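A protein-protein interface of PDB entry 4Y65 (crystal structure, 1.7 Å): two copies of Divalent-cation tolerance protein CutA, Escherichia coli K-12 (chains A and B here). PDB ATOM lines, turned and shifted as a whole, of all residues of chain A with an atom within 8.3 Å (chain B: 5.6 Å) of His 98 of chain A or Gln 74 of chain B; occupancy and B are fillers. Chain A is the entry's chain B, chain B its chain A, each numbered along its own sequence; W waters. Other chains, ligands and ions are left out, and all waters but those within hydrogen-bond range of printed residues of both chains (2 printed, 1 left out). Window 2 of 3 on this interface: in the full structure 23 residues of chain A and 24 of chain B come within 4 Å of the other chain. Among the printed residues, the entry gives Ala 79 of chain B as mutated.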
ATOM      1  N   SER A   6      28.213  15.607  -8.108  1.00  0.00           N
ATOM      2  CA  SER A   6      27.176  14.579  -8.137  1.00  0.00           C
ATOM      3  C   SER A   6      25.966  15.030  -7.314  1.00  0.00           C
ATOM      4  O   SER A   6      26.108  15.520  -6.189  1.00  0.00           O
ATOM      5  CB  SER A   6      27.733  13.273  -7.579  1.00  0.00           C
ATOM      6  OG  SER A   6      28.181  13.458  -6.251  1.00  0.00           O
ATOM      7  N   SER A   7      24.780  14.878  -7.892  1.00  0.00           N
ATOM      8  CA  SER A   7      23.541  15.267  -7.229  1.00  0.00           C
ATOM      9  C   SER A   7      22.542  14.120  -7.244  1.00  0.00           C
ATOM     10  O   SER A   7      22.444  13.383  -8.222  1.00  0.00           O
ATOM     11  CB  SER A   7      22.921  16.480  -7.917  1.00  0.00           C
ATOM     12  OG  SER A   7      21.637  16.762  -7.387  1.00  0.00           O
ATOM     13  N   ASN A   8      21.793  13.994  -6.157  1.00  0.00           N
ATOM     14  CA  ASN A   8      20.808  12.931  -6.015  1.00  0.00           C
ATOM     15  C   ASN A   8      19.374  13.440  -6.088  1.00  0.00           C
ATOM     16  O   ASN A   8      18.441  12.654  -5.956  1.00  0.00           O
ATOM     17  CB  ASN A   8      20.990  12.207  -4.668  1.00  0.00           C
ATOM     18  CG  ASN A   8      22.413  11.725  -4.436  1.00  0.00           C
ATOM     19  OD1 ASN A   8      23.079  12.175  -3.502  1.00  0.00           O
ATOM     20  ND2 ASN A   8      22.877  10.795  -5.267  1.00  0.00           N
ATOM     21  N   THR A   9      19.199  14.740  -6.305  1.00  0.00           N
ATOM     22  CA  THR A   9      17.863  15.320  -6.343  1.00  0.00           C
ATOM     23  C   THR A   9      17.753  16.547  -7.235  1.00  0.00           C
ATOM     24  O   THR A   9      18.730  17.271  -7.453  1.00  0.00           O
ATOM     25  CB  THR A   9      17.393  15.716  -4.916  1.00  0.00           C
ATOM     26  OG1 THR A   9      16.108  16.348  -4.983  1.00  0.00           O
ATOM     27  CG2 THR A   9      18.386  16.695  -4.270  1.00  0.00           C
ATOM     28  N   ALA A  10      16.547  16.769  -7.743  1.00  0.00           N
ATOM     29  CA  ALA A  10      16.265  17.903  -8.607  1.00  0.00           C
ATOM     30  C   ALA A  10      15.754  19.081  -7.787  1.00  0.00           C
ATOM     31  O   ALA A  10      15.342  20.104  -8.343  1.00  0.00           O
ATOM     32  CB  ALA A  10      15.233  17.509  -9.654  1.00  0.00           C
ATOM     33  N   SER A  11      15.768  18.939  -6.465  1.00  0.00           N
ATOM     34  CA  SER A  11      15.298  20.021  -5.606  1.00  0.00           C
ATOM     35  C   SER A  11      16.265  21.197  -5.641  1.00  0.00           C
ATOM     36  O   SER A  11      17.451  21.045  -5.944  1.00  0.00           O
ATOM     37  CB  SER A  11      15.112  19.536  -4.162  1.00  0.00           C
ATOM     38  OG  SER A  11      16.322  19.051  -3.611  1.00  0.00           O
ATOM     39  N   PRO A  95      21.395  25.335  -6.038  1.00  0.00           N
ATOM     40  CA  PRO A  95      21.199  23.891  -6.186  1.00  0.00           C
ATOM     41  C   PRO A  95      21.343  23.083  -4.905  1.00  0.00           C
ATOM     42  O   PRO A  95      22.181  23.386  -4.061  1.00  0.00           O
ATOM     43  CB  PRO A  95      22.266  23.511  -7.204  1.00  0.00           C
ATOM     44  CG  PRO A  95      23.399  24.387  -6.794  1.00  0.00           C
ATOM     45  CD  PRO A  95      22.722  25.734  -6.545  1.00  0.00           C
ATOM     46  N   VAL A  96      20.501  22.065  -4.767  1.00  0.00           N
ATOM     47  CA  VAL A  96      20.548  21.159  -3.626  1.00  0.00           C
ATOM     48  C   VAL A  96      21.132  19.882  -4.217  1.00  0.00           C
ATOM     49  O   VAL A  96      20.583  19.338  -5.174  1.00  0.00           O
ATOM     50  CB  VAL A  96      19.144  20.851  -3.071  1.00  0.00           C
ATOM     51  CG1 VAL A  96      19.233  19.742  -2.012  1.00  0.00           C
ATOM     52  CG2 VAL A  96      18.526  22.116  -2.483  1.00  0.00           C
ATOM     53  N   THR A  97      22.247  19.417  -3.666  1.00  0.00           N
ATOM     54  CA  THR A  97      22.887  18.211  -4.173  1.00  0.00           C
ATOM     55  C   THR A  97      22.425  16.951  -3.458  1.00  0.00           C
ATOM     56  O   THR A  97      22.430  15.863  -4.034  1.00  0.00           O
ATOM     57  CB  THR A  97      24.424  18.310  -4.069  1.00  0.00           C
ATOM     58  OG1 THR A  97      24.790  18.712  -2.745  1.00  0.00           O
ATOM     59  CG2 THR A  97      24.962  19.315  -5.073  1.00  0.00           C
ATOM     60  N   HIS A  98      22.009  17.096  -2.208  1.00  0.00           N
ATOM     61  CA  HIS A  98      21.559  15.949  -1.435  1.00  0.00           C
ATOM     62  C   HIS A  98      20.603  16.398  -0.341  1.00  0.00           C
ATOM     63  O   HIS A  98      20.538  17.578  -0.004  1.00  0.00           O
ATOM     64  CB  HIS A  98      22.770  15.239  -0.818  1.00  0.00           C
ATOM     65  CG  HIS A  98      22.429  13.976  -0.094  1.00  0.00           C
ATOM     66  ND1 HIS A  98      21.680  12.969  -0.665  1.00  0.00           N
ATOM     67  CD2 HIS A  98      22.747  13.547   1.150  1.00  0.00           C
ATOM     68  CE1 HIS A  98      21.552  11.974   0.196  1.00  0.00           C
ATOM     69  NE2 HIS A  98      22.191  12.300   1.305  1.00  0.00           N
ATOM     70  N   GLY A  99      19.849  15.455   0.204  1.00  0.00           N
ATOM     71  CA  GLY A  99      18.928  15.792   1.268  1.00  0.00           C
ATOM     72  C   GLY A  99      18.342  14.532   1.855  1.00  0.00           C
ATOM     73  O   GLY A  99      18.535  13.441   1.317  1.00  0.00           O
ATOM     74  N   ASP A 100      17.636  14.675   2.966  1.00  0.00           N
ATOM     75  CA  ASP A 100      17.013  13.527   3.603  1.00  0.00           C
ATOM     76  C   ASP A 100      15.942  12.977   2.664  1.00  0.00           C
ATOM     77  O   ASP A 100      15.118  13.729   2.148  1.00  0.00           O
ATOM     78  CB  ASP A 100      16.370  13.935   4.915  1.00  0.00           C
ATOM     79  CG  ASP A 100      15.537  12.830   5.502  1.00  0.00           C
ATOM     80  OD1 ASP A 100      16.132  11.836   5.973  1.00  0.00           O
ATOM     81  OD2 ASP A 100      14.298  12.949   5.469  1.00  0.00           O
ATOM     82  N   THR A 101      15.950  11.667   2.453  1.00  0.00           N
ATOM     83  CA  THR A 101      14.989  11.048   1.544  1.00  0.00           C
ATOM     84  C   THR A 101      13.519  11.299   1.872  1.00  0.00           C
ATOM     85  O   THR A 101      12.716  11.532   0.969  1.00  0.00           O
ATOM     86  CB  THR A 101      15.229   9.534   1.445  1.00  0.00           C
ATOM     87  OG1 THR A 101      15.087   8.940   2.738  1.00  0.00           O
ATOM     88  CG2 THR A 101      16.629   9.258   0.914  1.00  0.00           C
ATOM     89  N   TYR A 103      12.225  13.858   3.579  1.00  0.00           N
ATOM     90  CA  TYR A 103      11.909  15.258   3.355  1.00  0.00           C
ATOM     91  C   TYR A 103      11.776  15.546   1.864  1.00  0.00           C
ATOM     92  O   TYR A 103      10.863  16.252   1.442  1.00  0.00           O
ATOM     93  CB  TYR A 103      12.988  16.163   3.951  1.00  0.00           C
ATOM     94  CG  TYR A 103      12.673  17.633   3.783  1.00  0.00           C
ATOM     95  CD1 TYR A 103      11.639  18.228   4.501  1.00  0.00           C
ATOM     96  CD2 TYR A 103      13.370  18.417   2.867  1.00  0.00           C
ATOM     97  CE1 TYR A 103      11.302  19.563   4.310  1.00  0.00           C
ATOM     98  CE2 TYR A 103      13.039  19.759   2.665  1.00  0.00           C
ATOM     99  CZ  TYR A 103      12.002  20.322   3.393  1.00  0.00           C
ATOM    100  OH  TYR A 103      11.666  21.644   3.211  1.00  0.00           O
ATOM    101  N   LEU A 104      12.685  14.995   1.064  1.00  0.00           N
ATOM    102  CA  LEU A 104      12.653  15.235  -0.379  1.00  0.00           C
ATOM    103  C   LEU A 104      11.429  14.607  -1.025  1.00  0.00           C
ATOM    104  O   LEU A 104      10.884  15.137  -1.993  1.00  0.00           O
ATOM    105  CB  LEU A 104      13.930  14.702  -1.037  1.00  0.00           C
ATOM    106  CG  LEU A 104      15.223  15.452  -0.698  1.00  0.00           C
ATOM    107  CD1 LEU A 104      16.391  14.770  -1.395  1.00  0.00           C
ATOM    108  CD2 LEU A 104      15.125  16.914  -1.146  1.00  0.00           C
ATOM    109  N   VAL B  70      31.303  16.570   1.734  1.00  0.00           N
ATOM    110  CA  VAL B  70      30.570  15.478   1.103  1.00  0.00           C
ATOM    111  C   VAL B  70      30.841  14.158   1.827  1.00  0.00           C
ATOM    112  O   VAL B  70      29.944  13.332   1.978  1.00  0.00           O
ATOM    113  CB  VAL B  70      30.957  15.345  -0.390  1.00  0.00           C
ATOM    114  CG1 VAL B  70      30.323  14.100  -0.994  1.00  0.00           C
ATOM    115  CG2 VAL B  70      30.484  16.579  -1.148  1.00  0.00           C
ATOM    116  N   SER B  71      32.074  13.981   2.290  1.00  0.00           N
ATOM    117  CA  SER B  71      32.460  12.766   2.996  1.00  0.00           C
ATOM    118  C   SER B  71      31.602  12.493   4.226  1.00  0.00           C
ATOM    119  O   SER B  71      31.341  11.338   4.568  1.00  0.00           O
ATOM    120  CB  SER B  71      33.926  12.843   3.429  1.00  0.00           C
ATOM    121  OG  SER B  71      34.786  12.986   2.311  1.00  0.00           O
ATOM    122  N   HIS B  72      31.158  13.551   4.892  1.00  0.00           N
ATOM    123  CA  HIS B  72      30.354  13.385   6.100  1.00  0.00           C
ATOM    124  C   HIS B  72      28.882  13.764   5.988  1.00  0.00           C
ATOM    125  O   HIS B  72      28.134  13.577   6.943  1.00  0.00           O
ATOM    126  CB  HIS B  72      30.971  14.198   7.235  1.00  0.00           C
ATOM    127  CG  HIS B  72      32.389  13.834   7.535  1.00  0.00           C
ATOM    128  ND1 HIS B  72      33.453  14.284   6.783  1.00  0.00           N
ATOM    129  CD2 HIS B  72      32.919  13.055   8.507  1.00  0.00           C
ATOM    130  CE1 HIS B  72      34.577  13.802   7.280  1.00  0.00           C
ATOM    131  NE2 HIS B  72      34.281  13.053   8.327  1.00  0.00           N
ATOM    132  N   GLN B  73      28.454  14.281   4.838  1.00  0.00           N
ATOM    133  CA  GLN B  73      27.060  14.713   4.705  1.00  0.00           C
ATOM    134  C   GLN B  73      26.011  13.664   5.041  1.00  0.00           C
ATOM    135  O   GLN B  73      25.022  13.966   5.709  1.00  0.00           O
ATOM    136  CB  GLN B  73      26.785  15.271   3.302  1.00  0.00           C
ATOM    137  CG  GLN B  73      26.949  14.265   2.176  1.00  0.00           C
ATOM    138  CD  GLN B  73      26.725  14.894   0.818  1.00  0.00           C
ATOM    139  OE1 GLN B  73      27.199  16.000   0.548  1.00  0.00           O
ATOM    140  NE2 GLN B  73      26.018  14.188  -0.049  1.00  0.00           N
ATOM    141  N   GLN B  74      26.222  12.435   4.581  1.00  0.00           N
ATOM    142  CA  GLN B  74      25.277  11.358   4.839  1.00  0.00           C
ATOM    143  C   GLN B  74      25.150  11.084   6.338  1.00  0.00           C
ATOM    144  O   GLN B  74      24.041  11.050   6.877  1.00  0.00           O
ATOM    145  CB  GLN B  74      25.727  10.086   4.114  1.00  0.00           C
ATOM    146  CG  GLN B  74      24.716   8.957   4.159  1.00  0.00           C
ATOM    147  CD  GLN B  74      23.390   9.338   3.528  1.00  0.00           C
ATOM    148  OE1 GLN B  74      23.348   9.881   2.420  1.00  0.00           O
ATOM    149  NE2 GLN B  74      22.297   9.049   4.226  1.00  0.00           N
ATOM    150  N   ALA B  75      26.288  10.892   7.005  1.00  0.00           N
ATOM    151  CA  ALA B  75      26.299  10.628   8.439  1.00  0.00           C
ATOM    152  C   ALA B  75      25.692  11.801   9.201  1.00  0.00           C
ATOM    153  O   ALA B  75      24.949  11.606  10.162  1.00  0.00           O
ATOM    154  CB  ALA B  75      27.725  10.369   8.921  1.00  0.00           C
ATOM    155  N   LEU B  76      26.012  13.021   8.781  1.00  0.00           N
ATOM    156  CA  LEU B  76      25.459  14.193   9.449  1.00  0.00           C
ATOM    157  C   LEU B  76      23.939  14.197   9.355  1.00  0.00           C
ATOM    158  O   LEU B  76      23.255  14.413  10.351  1.00  0.00           O
ATOM    159  CB  LEU B  76      26.006  15.485   8.831  1.00  0.00           C
ATOM    160  CG  LEU B  76      25.439  16.803   9.377  1.00  0.00           C
ATOM    161  CD1 LEU B  76      25.730  16.938  10.875  1.00  0.00           C
ATOM    162  CD2 LEU B  76      26.052  17.967   8.617  1.00  0.00           C
ATOM    163  N   LEU B  77      23.409  13.960   8.158  1.00  0.00           N
ATOM    164  CA  LEU B  77      21.960  13.960   7.984  1.00  0.00           C
ATOM    165  C   LEU B  77      21.270  12.904   8.835  1.00  0.00           C
ATOM    166  O   LEU B  77      20.236  13.173   9.445  1.00  0.00           O
ATOM    167  CB  LEU B  77      21.588  13.766   6.509  1.00  0.00           C
ATOM    168  CG  LEU B  77      22.003  14.878   5.537  1.00  0.00           C
ATOM    169  CD1 LEU B  77      21.482  14.550   4.145  1.00  0.00           C
ATOM    170  CD2 LEU B  77      21.457  16.213   6.007  1.00  0.00           C
ATOM    171  N   GLU B  78      21.840  11.704   8.878  1.00  0.00           N
ATOM    172  CA  GLU B  78      21.258  10.617   9.660  1.00  0.00           C
ATOM    173  C   GLU B  78      21.289  10.967  11.146  1.00  0.00           C
ATOM    174  O   GLU B  78      20.344  10.674  11.881  1.00  0.00           O
ATOM    175  CB  GLU B  78      22.016   9.303   9.388  1.00  0.00           C
ATOM    176  CG  GLU B  78      22.026   8.913   7.904  1.00  0.00           C
ATOM    177  CD  GLU B  78      22.834   7.658   7.598  1.00  0.00           C
ATOM    178  OE1 GLU B  78      23.759   7.333   8.372  1.00  0.00           O
ATOM    179  OE2 GLU B  78      22.556   7.003   6.571  1.00  0.00           O
ATOM    180  N   ALA B  79      22.366  11.616  11.581  1.00  0.00           N
ATOM    181  CA  ALA B  79      22.499  12.011  12.982  1.00  0.00           C
ATOM    182  C   ALA B  79      21.468  13.078  13.345  1.00  0.00           C
ATOM    183  O   ALA B  79      20.810  12.992  14.383  1.00  0.00           O
ATOM    184  CB  ALA B  79      23.907  12.534  13.257  1.00  0.00           C
ATOM    185  N   LEU B  91      16.143  18.919   5.807  1.00  0.00           N
ATOM    186  CA  LEU B  91      17.560  18.583   5.816  1.00  0.00           C
ATOM    187  C   LEU B  91      18.005  18.608   4.364  1.00  0.00           C
ATOM    188  O   LEU B  91      17.742  17.671   3.607  1.00  0.00           O
ATOM    189  CB  LEU B  91      17.787  17.194   6.419  1.00  0.00           C
ATOM    190  CG  LEU B  91      17.473  17.040   7.913  1.00  0.00           C
ATOM    191  CD1 LEU B  91      17.560  15.577   8.323  1.00  0.00           C
ATOM    192  CD2 LEU B  91      18.455  17.873   8.722  1.00  0.00           C
ATOM    193  N   LEU B  92      18.670  19.694   3.983  1.00  0.00           N
ATOM    194  CA  LEU B  92      19.125  19.883   2.613  1.00  0.00           C
ATOM    195  C   LEU B  92      20.609  20.208   2.547  1.00  0.00           C
ATOM    196  O   LEU B  92      21.143  20.883   3.426  1.00  0.00           O
ATOM    197  CB  LEU B  92      18.325  21.017   1.970  1.00  0.00           C
ATOM    198  CG  LEU B  92      16.807  20.826   1.937  1.00  0.00           C
ATOM    199  CD1 LEU B  92      16.137  22.146   1.580  1.00  0.00           C
ATOM    200  CD2 LEU B  92      16.442  19.732   0.926  1.00  0.00           C
ATOM    201  N   VAL B  93      21.274  19.738   1.495  1.00  0.00           N
ATOM    202  CA  VAL B  93      22.701  19.987   1.340  1.00  0.00           C
ATOM    203  C   VAL B  93      22.977  20.840   0.112  1.00  0.00           C
ATOM    204  O   VAL B  93      22.534  20.511  -0.981  1.00  0.00           O
ATOM    205  CB  VAL B  93      23.483  18.659   1.200  1.00  0.00           C
ATOM    206  CG1 VAL B  93      24.976  18.945   1.071  1.00  0.00           C
ATOM    207  CG2 VAL B  93      23.195  17.751   2.405  1.00  0.00           C
ATOM    208  N   LEU B  94      23.698  21.940   0.305  1.00  0.00           N
ATOM    209  CA  LEU B  94      24.056  22.833  -0.796  1.00  0.00           C
ATOM    210  C   LEU B  94      25.568  22.762  -1.019  1.00  0.00           C
ATOM    211  O   LEU B  94      26.345  22.734  -0.067  1.00  0.00           O
ATOM    212  CB  LEU B  94      23.667  24.275  -0.471  1.00  0.00           C
ATOM    213  CG  LEU B  94      22.208  24.591  -0.134  1.00  0.00           C
ATOM    214  CD1 LEU B  94      22.090  26.077   0.156  1.00  0.00           C
ATOM    215  CD2 LEU B  94      21.301  24.203  -1.279  1.00  0.00           C
HETATM  216  O   HOH W   1      20.490  11.137   3.969  1.00  0.00           O
HETATM  217  O   HOH W   2      26.697  17.103  -1.881  1.00  0.00           O
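The side-chain amide nitrogen (NE2) of Gln 74 of chain B lies within hydrogen-bond range of the side-chain carboxylate (OE2) of Glu 78 of chain B (3.1 Å).
N of Asn 8 of chain A is in hydrogen-bond range of O of Thr 97 of chain A (2.9 Å).
OD1 of Asn 8 of chain A is in hydrogen-bond range of ND1 of His 98 of chain A.
O of Ser 11 of chain A sits close to N of Val 96 of chain A, 3.4 Å away.
The backbone NH (N) of Tyr 103 of chain A lies within hydrogen-bond range of the side-chain carboxylate (OD2) of Asp 100 of chain A, 2.9 Å away.
Among the printed residues, pairs that only touch across the chains: Pro 95 of chain A with Leu 94 of chain B (3.0 Å), Val 96 of chain A with Val 93 of chain B (3.4 Å), Val 96 of chain A with Leu 94 of chain B (3.7 Å), His 98 of chain A with Gln 73 of chain B (3.5 Å), His 98 of chain A with Leu 77 of chain B (3.4 Å), His 98 of chain A with Leu 92 of chain B (3.7 Å), Gly 99 of chain A with Leu 77 of chain B (3.9 Å), Gly 99 of chain A with Leu 91 of chain B (3.2 Å), Tyr 103 of chain A with Leu 92 of chain B (3.8 Å) and Leu 104 of chain A with Leu 92 of chain B (3.7 Å).
No position is printed for both chains.
Of the 14 pairs that touch across the chains among the printed residues, none has its exchanged pair printed and touching as well.
NE2 of His 98 of chain A is in hydrogen-bond range of OE1 of Gln 74 of chain B, at 2.9 Å.
The backbone NH (N) of Asp 100 of chain A lies within hydrogen-bond range of the backbone carbonyl oxygen (O) of Leu 91 of chain B (3.1 Å).
The backbone NH (N) of Thr 97 of chain A lies within hydrogen-bond range of the backbone carbonyl oxygen (O) of Val 93 of chain B (2.9 Å).
O of His 98 of chain A sits at hydrogen-bond distance from N of Val 93 of chain B.
Of the 14 printed residues of chain B, 7 touch a printed residue of chain A.
Of the 15 printed residues of chain A, 8 touch a printed residue of chain B.
Hydrophobic or aromatic side chains of chain A that line the printed part of chain B: Val 96, His 98, Tyr 103 and Leu 104.
Ser 6 of chain A touches none of the printed residues of chain B.
Printed residues of chain B within 4 Å of Pro 95 of chain A: Leu 94 (3.0 Å).
Printed residues of chain B within 4 Å of Thr 97 of chain A: Val 93 (2.9 Å).
Of chain B, only Gln 73 (3.5 Å), Gln 74 (2.9 Å), Leu 77 (3.4 Å), Leu 92 (3.7 Å) and Val 93 (2.7 Å) come within 4 Å of His 98 of chain A.
Val 70 of chain B touches none of the printed residues of chain A.
Printed residues of chain A within 4 Å of Gln 73 of chain B: His 98.
No residue of chain A comes within 4 Å of Ala 75 of chain B.
Printed residues of chain A within 4 Å of Leu 94 of chain B: Pro 95 (3.0 Å) and Val 96 (3.7 Å).
The nearest residue of chain B that does not touch His 98 of chain A is Leu 91 of chain B (4.6 Å).
The nearest printed residue of chain A that does not touch Leu 91 of chain B is Tyr 103 of chain A (4.1 Å).
Water W2 lies within hydrogen-bond range of the side-chain hydroxyl (OG1) of Thr 97 of chain A (2.6 Å) and the side-chain amide oxygen (OE1) of Gln 73 of chain B (2.7 Å).
Water W1 lies within hydrogen-bond range of NE2 of Gln 74 of chain B (2.8 Å) and NE2 of His 98 of chain A (3.4 Å).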
